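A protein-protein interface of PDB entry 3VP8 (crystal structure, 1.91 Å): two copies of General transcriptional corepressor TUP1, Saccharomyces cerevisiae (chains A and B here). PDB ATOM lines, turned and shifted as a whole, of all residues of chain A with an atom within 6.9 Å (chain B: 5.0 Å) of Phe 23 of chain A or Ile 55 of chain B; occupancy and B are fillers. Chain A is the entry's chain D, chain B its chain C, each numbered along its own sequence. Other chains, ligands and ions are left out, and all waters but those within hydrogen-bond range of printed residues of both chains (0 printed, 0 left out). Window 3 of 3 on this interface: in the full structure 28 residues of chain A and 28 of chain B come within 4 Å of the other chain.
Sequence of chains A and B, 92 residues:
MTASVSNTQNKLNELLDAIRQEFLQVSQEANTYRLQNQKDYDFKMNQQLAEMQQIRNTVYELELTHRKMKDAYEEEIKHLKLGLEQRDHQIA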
ATOM      1  N   ALA A  18      12.424  13.604   9.564  1.00  0.00           N
ATOM      2  CA  ALA A  18      12.931  13.736   8.200  1.00  0.00           C
ATOM      3  C   ALA A  18      13.996  14.827   8.131  1.00  0.00           C
ATOM      4  O   ALA A  18      15.063  14.637   7.543  1.00  0.00           O
ATOM      5  CB  ALA A  18      11.800  14.021   7.213  1.00  0.00           C
ATOM      6  N   ILE A  19      13.726  15.968   8.751  1.00  0.00           N
ATOM      7  CA  ILE A  19      14.681  17.059   8.659  1.00  0.00           C
ATOM      8  C   ILE A  19      15.985  16.682   9.352  1.00  0.00           C
ATOM      9  O   ILE A  19      17.068  17.038   8.898  1.00  0.00           O
ATOM     10  CB  ILE A  19      14.115  18.384   9.204  1.00  0.00           C
ATOM     11  CG1 ILE A  19      14.581  19.536   8.312  1.00  0.00           C
ATOM     12  CG2 ILE A  19      14.538  18.608  10.646  1.00  0.00           C
ATOM     13  CD1 ILE A  19      14.091  20.889   8.746  1.00  0.00           C
ATOM     14  N   ARG A  20      15.879  15.933  10.441  1.00  0.00           N
ATOM     15  CA  ARG A  20      17.061  15.502  11.170  1.00  0.00           C
ATOM     16  C   ARG A  20      17.938  14.600  10.310  1.00  0.00           C
ATOM     17  O   ARG A  20      19.177  14.735  10.292  1.00  0.00           O
ATOM     18  CB  ARG A  20      16.657  14.782  12.459  1.00  0.00           C
ATOM     19  CG  ARG A  20      17.318  13.429  12.642  1.00  0.00           C
ATOM     20  CD  ARG A  20      18.135  13.364  13.922  1.00  0.00           C
ATOM     21  NE  ARG A  20      17.646  12.324  14.825  1.00  0.00           N
ATOM     22  CZ  ARG A  20      18.088  12.147  16.067  1.00  0.00           C
ATOM     23  NH1 ARG A  20      19.032  12.943  16.554  1.00  0.00           N
ATOM     24  NH2 ARG A  20      17.583  11.175  16.820  1.00  0.00           N
ATOM     25  N   GLN A  21      17.301  13.680   9.597  1.00  0.00           N
ATOM     26  CA  GLN A  21      18.043  12.777   8.720  1.00  0.00           C
ATOM     27  C   GLN A  21      18.673  13.546   7.565  1.00  0.00           C
ATOM     28  O   GLN A  21      19.783  13.228   7.122  1.00  0.00           O
ATOM     29  CB  GLN A  21      17.136  11.678   8.167  1.00  0.00           C
ATOM     30  CG  GLN A  21      17.856  10.747   7.217  1.00  0.00           C
ATOM     31  CD  GLN A  21      19.125  10.173   7.836  1.00  0.00           C
ATOM     32  OE1 GLN A  21      19.083   9.562   8.910  1.00  0.00           O
ATOM     33  NE2 GLN A  21      20.264  10.389   7.174  1.00  0.00           N
ATOM     34  N   GLU A  22      17.972  14.565   7.092  1.00  0.00           N
ATOM     35  CA  GLU A  22      18.453  15.358   5.961  1.00  0.00           C
ATOM     36  C   GLU A  22      19.721  16.122   6.328  1.00  0.00           C
ATOM     37  O   GLU A  22      20.688  16.149   5.560  1.00  0.00           O
ATOM     38  CB  GLU A  22      17.359  16.311   5.471  1.00  0.00           C
ATOM     39  CG  GLU A  22      16.220  15.599   4.794  1.00  0.00           C
ATOM     40  CD  GLU A  22      14.969  16.461   4.659  1.00  0.00           C
ATOM     41  OE1 GLU A  22      14.916  17.564   5.253  1.00  0.00           O
ATOM     42  OE2 GLU A  22      14.035  16.018   3.958  1.00  0.00           O
ATOM     43  N   PHE A  23      19.719  16.747   7.499  1.00  0.00           N
ATOM     44  CA  PHE A  23      20.896  17.460   7.971  1.00  0.00           C
ATOM     45  C   PHE A  23      22.048  16.503   8.177  1.00  0.00           C
ATOM     46  O   PHE A  23      23.197  16.841   7.923  1.00  0.00           O
ATOM     47  CB  PHE A  23      20.617  18.150   9.312  1.00  0.00           C
ATOM     48  CG  PHE A  23      19.811  19.401   9.194  1.00  0.00           C
ATOM     49  CD1 PHE A  23      18.680  19.591   9.980  1.00  0.00           C
ATOM     50  CD2 PHE A  23      20.194  20.403   8.316  1.00  0.00           C
ATOM     51  CE1 PHE A  23      17.937  20.756   9.877  1.00  0.00           C
ATOM     52  CE2 PHE A  23      19.445  21.578   8.210  1.00  0.00           C
ATOM     53  CZ  PHE A  23      18.328  21.750   8.990  1.00  0.00           C
ATOM     54  N   LEU A  24      21.759  15.316   8.690  1.00  0.00           N
ATOM     55  CA  LEU A  24      22.847  14.392   9.004  1.00  0.00           C
ATOM     56  C   LEU A  24      23.497  13.921   7.721  1.00  0.00           C
ATOM     57  O   LEU A  24      24.725  13.760   7.643  1.00  0.00           O
ATOM     58  CB  LEU A  24      22.323  13.194   9.793  1.00  0.00           C
ATOM     59  CG  LEU A  24      23.368  12.109  10.044  1.00  0.00           C
ATOM     60  CD1 LEU A  24      24.491  12.697  10.889  1.00  0.00           C
ATOM     61  CD2 LEU A  24      22.751  10.895  10.728  1.00  0.00           C
ATOM     62  N   GLN A  25      22.658  13.694   6.717  1.00  0.00           N
ATOM     63  CA  GLN A  25      23.110  13.263   5.410  1.00  0.00           C
ATOM     64  C   GLN A  25      24.014  14.313   4.757  1.00  0.00           C
ATOM     65  O   GLN A  25      24.976  13.973   4.049  1.00  0.00           O
ATOM     66  CB  GLN A  25      21.906  12.977   4.515  1.00  0.00           C
ATOM     67  CG  GLN A  25      22.242  12.680   3.046  1.00  0.00           C
ATOM     68  CD  GLN A  25      21.007  12.276   2.255  1.00  0.00           C
ATOM     69  OE1 GLN A  25      20.233  13.132   1.802  1.00  0.00           O
ATOM     70  NE2 GLN A  25      20.810  10.965   2.091  1.00  0.00           N
ATOM     71  N   VAL A  26      23.714  15.589   4.982  1.00  0.00           N
ATOM     72  CA  VAL A  26      24.547  16.654   4.415  1.00  0.00           C
ATOM     73  C   VAL A  26      25.918  16.691   5.080  1.00  0.00           C
ATOM     74  O   VAL A  26      26.940  16.922   4.423  1.00  0.00           O
ATOM     75  CB  VAL A  26      23.893  18.038   4.538  1.00  0.00           C
ATOM     76  CG1 VAL A  26      24.870  19.120   4.060  1.00  0.00           C
ATOM     77  CG2 VAL A  26      22.611  18.086   3.725  1.00  0.00           C
ATOM     78  N   SER A  27      25.932  16.469   6.392  1.00  0.00           N
ATOM     79  CA  SER A  27      27.177  16.440   7.153  1.00  0.00           C
ATOM     80  C   SER A  27      28.024  15.198   6.855  1.00  0.00           C
ATOM     81  O   SER A  27      29.239  15.287   6.784  1.00  0.00           O
ATOM     82  CB  SER A  27      26.890  16.511   8.655  1.00  0.00           C
ATOM     83  OG  SER A  27      26.552  17.834   9.019  1.00  0.00           O
ATOM     84  N   GLN A  28      27.399  14.036   6.718  1.00  0.00           N
ATOM     85  CA  GLN A  28      28.150  12.823   6.405  1.00  0.00           C
ATOM     86  C   GLN A  28      28.749  12.899   4.997  1.00  0.00           C
ATOM     87  O   GLN A  28      29.882  12.469   4.761  1.00  0.00           O
ATOM     88  CB  GLN A  28      27.239  11.591   6.526  1.00  0.00           C
ATOM     89  CG  GLN A  28      26.891  11.196   7.963  1.00  0.00           C
ATOM     90  CD  GLN A  28      25.951   9.990   8.030  1.00  0.00           C
ATOM     91  OE1 GLN A  28      25.307   9.620   7.038  1.00  0.00           O
ATOM     92  NE2 GLN A  28      25.871   9.375   9.205  1.00  0.00           N
ATOM     93  N   GLU B  51      19.600  18.964  -1.849  1.00  0.00           N
ATOM     94  CA  GLU B  51      19.382  18.605  -0.442  1.00  0.00           C
ATOM     95  C   GLU B  51      18.877  19.804   0.378  1.00  0.00           C
ATOM     96  O   GLU B  51      17.970  19.675   1.215  1.00  0.00           O
ATOM     97  CB  GLU B  51      20.683  18.021   0.141  1.00  0.00           C
ATOM     98  CG  GLU B  51      21.075  16.724  -0.544  1.00  0.00           C
ATOM     99  CD  GLU B  51      22.462  16.217  -0.155  1.00  0.00           C
ATOM    100  OE1 GLU B  51      22.715  15.007  -0.360  1.00  0.00           O
ATOM    101  OE2 GLU B  51      23.296  17.021   0.336  1.00  0.00           O
ATOM    102  N   MET B  52      19.446  20.976   0.113  1.00  0.00           N
ATOM    103  CA  MET B  52      19.034  22.209   0.802  1.00  0.00           C
ATOM    104  C   MET B  52      17.634  22.647   0.375  1.00  0.00           C
ATOM    105  O   MET B  52      16.878  23.192   1.172  1.00  0.00           O
ATOM    106  CB  MET B  52      20.043  23.345   0.561  1.00  0.00           C
ATOM    107  CG  MET B  52      21.430  23.053   1.123  1.00  0.00           C
ATOM    108  SD  MET B  52      21.447  22.592   2.881  1.00  0.00           S
ATOM    109  CE  MET B  52      20.971  24.156   3.607  1.00  0.00           C
ATOM    110  N   GLN B  53      17.297  22.402  -0.888  1.00  0.00           N
ATOM    111  CA  GLN B  53      15.957  22.681  -1.403  1.00  0.00           C
ATOM    112  C   GLN B  53      14.970  21.784  -0.671  1.00  0.00           C
ATOM    113  O   GLN B  53      13.909  22.239  -0.223  1.00  0.00           O
ATOM    114  CB  GLN B  53      15.913  22.431  -2.920  1.00  0.00           C
ATOM    115  CG  GLN B  53      15.142  23.477  -3.724  1.00  0.00           C
ATOM    116  CD  GLN B  53      15.397  23.382  -5.229  1.00  0.00           C
ATOM    117  OE1 GLN B  53      15.198  22.328  -5.842  1.00  0.00           O
ATOM    118  NE2 GLN B  53      15.843  24.489  -5.830  1.00  0.00           N
ATOM    119  N   GLN B  54      15.336  20.511  -0.517  1.00  0.00           N
ATOM    120  CA  GLN B  54      14.464  19.541   0.153  1.00  0.00           C
ATOM    121  C   GLN B  54      14.242  19.885   1.633  1.00  0.00           C
ATOM    122  O   GLN B  54      13.124  19.780   2.138  1.00  0.00           O
ATOM    123  CB  GLN B  54      15.010  18.117   0.001  1.00  0.00           C
ATOM    124  CG  GLN B  54      14.296  17.086   0.857  1.00  0.00           C
ATOM    125  CD  GLN B  54      14.858  15.686   0.670  1.00  0.00           C
ATOM    126  OE1 GLN B  54      16.060  15.508   0.437  1.00  0.00           O
ATOM    127  NE2 GLN B  54      13.988  14.683   0.759  1.00  0.00           N
ATOM    128  N   ILE B  55      15.313  20.284   2.319  1.00  0.00           N
ATOM    129  CA  ILE B  55      15.223  20.756   3.695  1.00  0.00           C
ATOM    130  C   ILE B  55      14.286  21.964   3.781  1.00  0.00           C
ATOM    131  O   ILE B  55      13.382  22.002   4.623  1.00  0.00           O
ATOM    132  CB  ILE B  55      16.636  21.105   4.244  1.00  0.00           C
ATOM    133  CG1 ILE B  55      17.452  19.822   4.438  1.00  0.00           C
ATOM    134  CG2 ILE B  55      16.555  21.867   5.548  1.00  0.00           C
ATOM    135  CD1 ILE B  55      18.955  20.078   4.755  1.00  0.00           C
ATOM    136  N   ARG B  56      14.509  22.950   2.914  1.00  0.00           N
ATOM    137  CA  ARG B  56      13.665  24.151   2.840  1.00  0.00           C
ATOM    138  C   ARG B  56      12.182  23.819   2.671  1.00  0.00           C
ATOM    139  O   ARG B  56      11.320  24.438   3.307  1.00  0.00           O
ATOM    140  CB  ARG B  56      14.119  25.055   1.676  1.00  0.00           C
ATOM    141  CG  ARG B  56      13.283  26.335   1.496  1.00  0.00           C
ATOM    142  CD  ARG B  56      13.628  27.107   0.211  1.00  0.00           C
ATOM    143  NE  ARG B  56      13.445  26.300  -0.999  1.00  0.00           N
ATOM    144  CZ  ARG B  56      13.346  26.791  -2.234  1.00  0.00           C
ATOM    145  NH1 ARG B  56      13.398  28.100  -2.441  1.00  0.00           N
ATOM    146  NH2 ARG B  56      13.188  25.968  -3.264  1.00  0.00           N
ATOM    147  N   ASN B  57      11.884  22.856   1.804  1.00  0.00           N
ATOM    148  CA  ASN B  57      10.500  22.430   1.607  1.00  0.00           C
ATOM    149  C   ASN B  57       9.935  21.702   2.824  1.00  0.00           C
ATOM    150  O   ASN B  57       8.750  21.850   3.152  1.00  0.00           O
ATOM    151  CB  ASN B  57      10.370  21.562   0.355  1.00  0.00           C
ATOM    152  CG  ASN B  57      10.260  22.388  -0.917  1.00  0.00           C
ATOM    153  OD1 ASN B  57      10.905  23.430  -1.056  1.00  0.00           O
ATOM    154  ND2 ASN B  57       9.407  21.944  -1.839  1.00  0.00           N
ATOM    155  N   THR B  58      10.778  20.921   3.496  1.00  0.00           N
ATOM    156  CA  THR B  58      10.365  20.255   4.730  1.00  0.00           C
ATOM    157  C   THR B  58      10.020  21.288   5.798  1.00  0.00           C
ATOM    158  O   THR B  58       9.012  21.156   6.490  1.00  0.00           O
ATOM    159  CB  THR B  58      11.431  19.302   5.239  1.00  0.00           C
ATOM    160  OG1 THR B  58      11.705  18.342   4.220  1.00  0.00           O
ATOM    161  CG2 THR B  58      10.950  18.569   6.485  1.00  0.00           C
ATOM    162  N   VAL B  59      10.836  22.330   5.919  1.00  0.00           N
ATOM    163  CA  VAL B  59      10.488  23.446   6.787  1.00  0.00           C
ATOM    164  C   VAL B  59       9.123  24.015   6.393  1.00  0.00           C
ATOM    165  O   VAL B  59       8.237  24.130   7.236  1.00  0.00           O
ATOM    166  CB  VAL B  59      11.546  24.555   6.757  1.00  0.00           C
ATOM    167  CG1 VAL B  59      11.032  25.805   7.469  1.00  0.00           C
ATOM    168  CG2 VAL B  59      12.827  24.072   7.404  1.00  0.00           C
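OE2 of Glu 22 of chain A lies close to NE2 of Gln 54 of chain B.
OG1 of Thr 58 of chain B sits at hydrogen-bond distance from OE2 of Glu 22 of chain A, 3.3 Å away.
The backbone carbonyl oxygen (O) of Gln 54 of chain B sits at hydrogen-bond distance from the side-chain hydroxyl (OG1) of Thr 58 of chain B, 2.9 Å away.
CD1 of Ile 19 of chain A touches CG2 of Val 59 of chain B, 3.7 Å away.
Ile 55 of chain B touches Glu 22 of chain A (CG1 to OE1, 3.5 Å).
Phe 23 of chain A touches Ile 55 of chain B (CD2 to CD1, 3.8 Å).
Glu 51 of chain B touches Gln 25 of chain A.
CG2 of Val 26 of chain A touches OE2 of Glu 51 of chain B (3.6 Å).
Of chain B, only Ile 55 comes within 4 Å of Phe 23 of chain A.
Of the printed residues of chain A, Ile 55 of chain B touches Glu 22 (3.5 Å) and Phe 23 (3.8 Å).
Printed residues of chain B within 4 Å of Val 26 of chain A: Glu 51.
Of the printed residues of chain B, Glu 22 of chain A touches Gln 54 (3.3 Å), Ile 55 (3.5 Å) and Thr 58 (3.3 Å).
Of the printed residues of chain A, Thr 58 of chain B touches Glu 22 (3.3 Å).
Gln 21 of chain A touches none of the printed residues of chain B.
The nearest printed residue of chain B that does not touch Phe 23 of chain A is Met 52 of chain B (5.5 Å).
The nearest residue of chain A that does not touch Ile 55 of chain B is Ile 19 of chain A (4.1 Å).
Of the 11 printed residues of chain A, 5 touch a printed residue of chain B.
Printed residues of chain A that touch a printed residue of chain B: Ile 19, Glu 22, Phe 23, Gln 25 and Val 26.
Among the printed residues, 7 pairs touch across the chains.
No position is printed for both chains.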
